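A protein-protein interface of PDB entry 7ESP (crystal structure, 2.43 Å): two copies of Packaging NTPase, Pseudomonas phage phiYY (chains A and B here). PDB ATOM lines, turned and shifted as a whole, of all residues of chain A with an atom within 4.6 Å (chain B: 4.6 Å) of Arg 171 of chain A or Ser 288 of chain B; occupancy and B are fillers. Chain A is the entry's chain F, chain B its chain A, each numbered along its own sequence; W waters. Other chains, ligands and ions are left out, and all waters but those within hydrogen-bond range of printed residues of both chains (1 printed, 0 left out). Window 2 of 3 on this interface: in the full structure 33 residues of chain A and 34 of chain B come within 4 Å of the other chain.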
ATOM      1  N   GLU A 170     -16.367  -4.540 -27.978  1.00  0.00           N
ATOM      2  CA  GLU A 170     -15.057  -4.649 -28.615  1.00  0.00           C
ATOM      3  C   GLU A 170     -14.328  -3.318 -28.541  1.00  0.00           C
ATOM      4  O   GLU A 170     -14.881  -2.308 -28.099  1.00  0.00           O
ATOM      5  CB  GLU A 170     -15.174  -4.992 -30.094  1.00  0.00           C
ATOM      6  CG  GLU A 170     -15.609  -6.340 -30.344  1.00  0.00           C
ATOM      7  CD  GLU A 170     -15.587  -6.636 -31.812  1.00  0.00           C
ATOM      8  OE1 GLU A 170     -16.073  -7.733 -32.179  1.00  0.00           O
ATOM      9  OE2 GLU A 170     -15.036  -5.810 -32.593  1.00  0.00           O
ATOM     10  N   ARG A 171     -13.085  -3.317 -29.043  1.00  0.00           N
ATOM     11  CA  ARG A 171     -12.340  -2.070 -29.145  1.00  0.00           C
ATOM     12  C   ARG A 171     -13.138  -1.030 -29.922  1.00  0.00           C
ATOM     13  O   ARG A 171     -13.208   0.137 -29.525  1.00  0.00           O
ATOM     14  CB  ARG A 171     -10.982  -2.301 -29.819  1.00  0.00           C
ATOM     15  CG  ARG A 171     -10.382  -0.981 -30.234  1.00  0.00           C
ATOM     16  CD  ARG A 171      -8.941  -1.012 -30.639  1.00  0.00           C
ATOM     17  NE  ARG A 171      -8.628  -2.009 -31.658  1.00  0.00           N
ATOM     18  CZ  ARG A 171      -9.079  -2.000 -32.909  1.00  0.00           C
ATOM     19  NH1 ARG A 171      -8.691  -2.961 -33.743  1.00  0.00           N
ATOM     20  NH2 ARG A 171      -9.924  -1.053 -33.328  1.00  0.00           N
ATOM     21  N   PHE A 172     -13.748  -1.452 -31.035  1.00  0.00           N
ATOM     22  CA  PHE A 172     -14.577  -0.571 -31.850  1.00  0.00           C
ATOM     23  C   PHE A 172     -15.621   0.169 -31.014  1.00  0.00           C
ATOM     24  O   PHE A 172     -15.798   1.381 -31.164  1.00  0.00           O
ATOM     25  CB  PHE A 172     -15.239  -1.392 -32.957  1.00  0.00           C
ATOM     26  CG  PHE A 172     -16.022  -0.568 -33.940  1.00  0.00           C
ATOM     27  CD1 PHE A 172     -15.367   0.146 -34.942  1.00  0.00           C
ATOM     28  CD2 PHE A 172     -17.418  -0.513 -33.869  1.00  0.00           C
ATOM     29  CE1 PHE A 172     -16.080   0.908 -35.871  1.00  0.00           C
ATOM     30  CE2 PHE A 172     -18.148   0.254 -34.785  1.00  0.00           C
ATOM     31  CZ  PHE A 172     -17.469   0.967 -35.797  1.00  0.00           C
ATOM     32  N   ASP A 173     -16.293  -0.528 -30.103  1.00  0.00           N
ATOM     33  CA  ASP A 173     -17.282   0.102 -29.232  1.00  0.00           C
ATOM     34  C   ASP A 173     -16.683   1.076 -28.235  1.00  0.00           C
ATOM     35  O   ASP A 173     -17.437   1.673 -27.454  1.00  0.00           O
ATOM     36  CB  ASP A 173     -18.073  -0.970 -28.476  1.00  0.00           C
ATOM     37  CG  ASP A 173     -18.729  -1.957 -29.415  1.00  0.00           C
ATOM     38  OD1 ASP A 173     -19.441  -1.518 -30.359  1.00  0.00           O
ATOM     39  OD2 ASP A 173     -18.502  -3.168 -29.239  1.00  0.00           O
ATOM     40  N   VAL A 174     -15.366   1.239 -28.208  1.00  0.00           N
ATOM     41  CA  VAL A 174     -14.736   2.238 -27.361  1.00  0.00           C
ATOM     42  C   VAL A 174     -14.278   3.441 -28.175  1.00  0.00           C
ATOM     43  O   VAL A 174     -14.430   4.579 -27.736  1.00  0.00           O
ATOM     44  CB  VAL A 174     -13.562   1.617 -26.572  1.00  0.00           C
ATOM     45  CG1 VAL A 174     -12.866   2.677 -25.685  1.00  0.00           C
ATOM     46  CG2 VAL A 174     -14.054   0.456 -25.737  1.00  0.00           C
ATOM     47  N   GLU A 175     -13.764   3.198 -29.380  1.00  0.00           N
ATOM     48  CA  GLU A 175     -13.141   4.222 -30.210  1.00  0.00           C
ATOM     49  C   GLU A 175     -13.977   4.667 -31.397  1.00  0.00           C
ATOM     50  O   GLU A 175     -13.985   5.858 -31.723  1.00  0.00           O
ATOM     51  CB  GLU A 175     -11.807   3.703 -30.745  1.00  0.00           C
ATOM     52  CG  GLU A 175     -10.986   2.969 -29.720  1.00  0.00           C
ATOM     53  CD  GLU A 175      -9.686   2.453 -30.303  1.00  0.00           C
ATOM     54  OE1 GLU A 175      -9.652   2.179 -31.536  1.00  0.00           O
ATOM     55  OE2 GLU A 175      -8.704   2.318 -29.529  1.00  0.00           O
ATOM     56  N   ASP B 134      -5.326  -5.785 -20.612  1.00  0.00           N
ATOM     57  CA  ASP B 134      -6.259  -5.008 -21.440  1.00  0.00           C
ATOM     58  C   ASP B 134      -7.514  -5.798 -21.806  1.00  0.00           C
ATOM     59  O   ASP B 134      -8.127  -5.529 -22.829  1.00  0.00           O
ATOM     60  CB  ASP B 134      -5.590  -4.486 -22.722  1.00  0.00           C
ATOM     61  CG  ASP B 134      -4.433  -3.531 -22.441  1.00  0.00           C
ATOM     62  OD1 ASP B 134      -4.316  -3.032 -21.299  1.00  0.00           O
ATOM     63  OD2 ASP B 134      -3.641  -3.273 -23.368  1.00  0.00           O
ATOM     64  N   MET B 136     -11.023  -6.685 -22.432  1.00  0.00           N
ATOM     65  CA  MET B 136     -12.312  -5.998 -22.493  1.00  0.00           C
ATOM     66  C   MET B 136     -13.150  -6.387 -21.279  1.00  0.00           C
ATOM     67  O   MET B 136     -13.124  -7.548 -20.865  1.00  0.00           O
ATOM     68  CB  MET B 136     -13.081  -6.367 -23.768  1.00  0.00           C
ATOM     69  CG  MET B 136     -12.587  -5.655 -25.015  1.00  0.00           C
ATOM     70  SD  MET B 136     -12.823  -3.853 -24.905  1.00  0.00           S
ATOM     71  CE  MET B 136     -14.609  -3.762 -25.043  1.00  0.00           C
ATOM     72  N   THR B 286      -9.548  -7.458 -26.442  1.00  0.00           N
ATOM     73  CA  THR B 286      -8.809  -6.518 -25.622  1.00  0.00           C
ATOM     74  C   THR B 286      -9.121  -5.092 -26.047  1.00  0.00           C
ATOM     75  O   THR B 286      -9.702  -4.843 -27.107  1.00  0.00           O
ATOM     76  CB  THR B 286      -7.299  -6.757 -25.729  1.00  0.00           C
ATOM     77  OG1 THR B 286      -6.867  -6.403 -27.050  1.00  0.00           O
ATOM     78  CG2 THR B 286      -6.947  -8.218 -25.451  1.00  0.00           C
ATOM     79  N   LEU B 287      -8.663  -4.150 -25.223  1.00  0.00           N
ATOM     80  CA  LEU B 287      -8.802  -2.729 -25.526  1.00  0.00           C
ATOM     81  C   LEU B 287      -8.050  -2.306 -26.777  1.00  0.00           C
ATOM     82  O   LEU B 287      -8.333  -1.231 -27.308  1.00  0.00           O
ATOM     83  CB  LEU B 287      -8.302  -1.891 -24.358  1.00  0.00           C
ATOM     84  CG  LEU B 287      -9.217  -2.014 -23.165  1.00  0.00           C
ATOM     85  CD1 LEU B 287      -8.565  -1.405 -21.937  1.00  0.00           C
ATOM     86  CD2 LEU B 287     -10.520  -1.343 -23.504  1.00  0.00           C
ATOM     87  N   SER B 288      -7.080  -3.092 -27.250  1.00  0.00           N
ATOM     88  CA  SER B 288      -6.344  -2.717 -28.451  1.00  0.00           C
ATOM     89  C   SER B 288      -6.585  -3.633 -29.644  1.00  0.00           C
ATOM     90  O   SER B 288      -6.144  -3.297 -30.748  1.00  0.00           O
ATOM     91  CB  SER B 288      -4.834  -2.640 -28.152  1.00  0.00           C
ATOM     92  OG  SER B 288      -4.318  -3.873 -27.669  1.00  0.00           O
ATOM     93  N   GLY B 289      -7.286  -4.761 -29.473  1.00  0.00           N
ATOM     94  CA  GLY B 289      -7.458  -5.700 -30.575  1.00  0.00           C
ATOM     95  C   GLY B 289      -7.889  -7.079 -30.114  1.00  0.00           C
ATOM     96  O   GLY B 289      -8.819  -7.177 -29.313  1.00  0.00           O
HETATM   97  O   HOH W   1     -11.643  -5.629 -28.894  1.00  0.00           O
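No position is printed for both chains.
Among the printed residues, merely in contact across the chains: Glu 170 of chain A with Met 136 of chain B (3.4 Å), Arg 171 of chain A with Thr 286 of chain B (3.9 Å), Arg 171 of chain A with Leu 287 of chain B (3.4 Å) and Arg 171 of chain A with Gly 289 of chain B (3.8 Å).
Water W1 lies within hydrogen-bond range of the backbone NH (N) of Arg 171 of chain A (2.7 Å), the backbone carbonyl oxygen (O) of Thr 286 of chain B (2.8 Å) and the backbone carbonyl oxygen (O) of Gly 289 of chain B (3.2 Å).
OG1 of Thr 286 of chain B lies close to N of Ser 288 of chain B. The side-chain hydroxyl (OG1) of Thr 286 of chain B sits at hydrogen-bond distance from the backbone NH (N) of Gly 289 of chain B. O of Asp 134 of chain B lies within hydrogen-bond range of N of Leu 287 of chain B, at 2.8 Å. The side-chain carboxylate (OD2) of Asp 173 of chain A is in hydrogen-bond range of the backbone NH (N) of Glu 170 of chain A, at 2.8 Å. The guanidinium group of Arg 171 of chain A is in salt-bridge range of the side-chain carboxylate of Glu 175 of chain A, at 3.7 Å.
Of chain B, only Thr 286, Leu 287, Ser 288 and Gly 289 come within 4 Å of Arg 171 of chain A. Ser 288 of chain B touches just one residue of chain A: Arg 171. Of the printed residues of chain A, Met 136 of chain B touches Glu 170 (3.4 Å). Printed residues of chain A within 4 Å of Thr 286 of chain B: Arg 171 (3.9 Å). Of the printed residues of chain A, Gly 289 of chain B touches Arg 171. Of the printed residues of chain B, Glu 170 of chain A touches Met 136 (3.4 Å). Asp 134 of chain B touches none of the printed residues of chain A. The nearest printed residue of chain A that does not touch Ser 288 of chain B is Glu 175 of chain A (5.7 Å).
Of the 6 printed residues of chain B, 5 touch a printed residue of chain A. Among the printed residues, 5 pairs touch across the chains. Among the printed residues, no Asp or Glu carboxylate lies within 4 Å of a Lys or Arg side-chain nitrogen of the other chain.
The backbone carbonyl oxygen (O) of Ser 288 of chain B lies within hydrogen-bond range of the guanidinium group (NE) of Arg 171 of chain A, 2.9 Å away.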
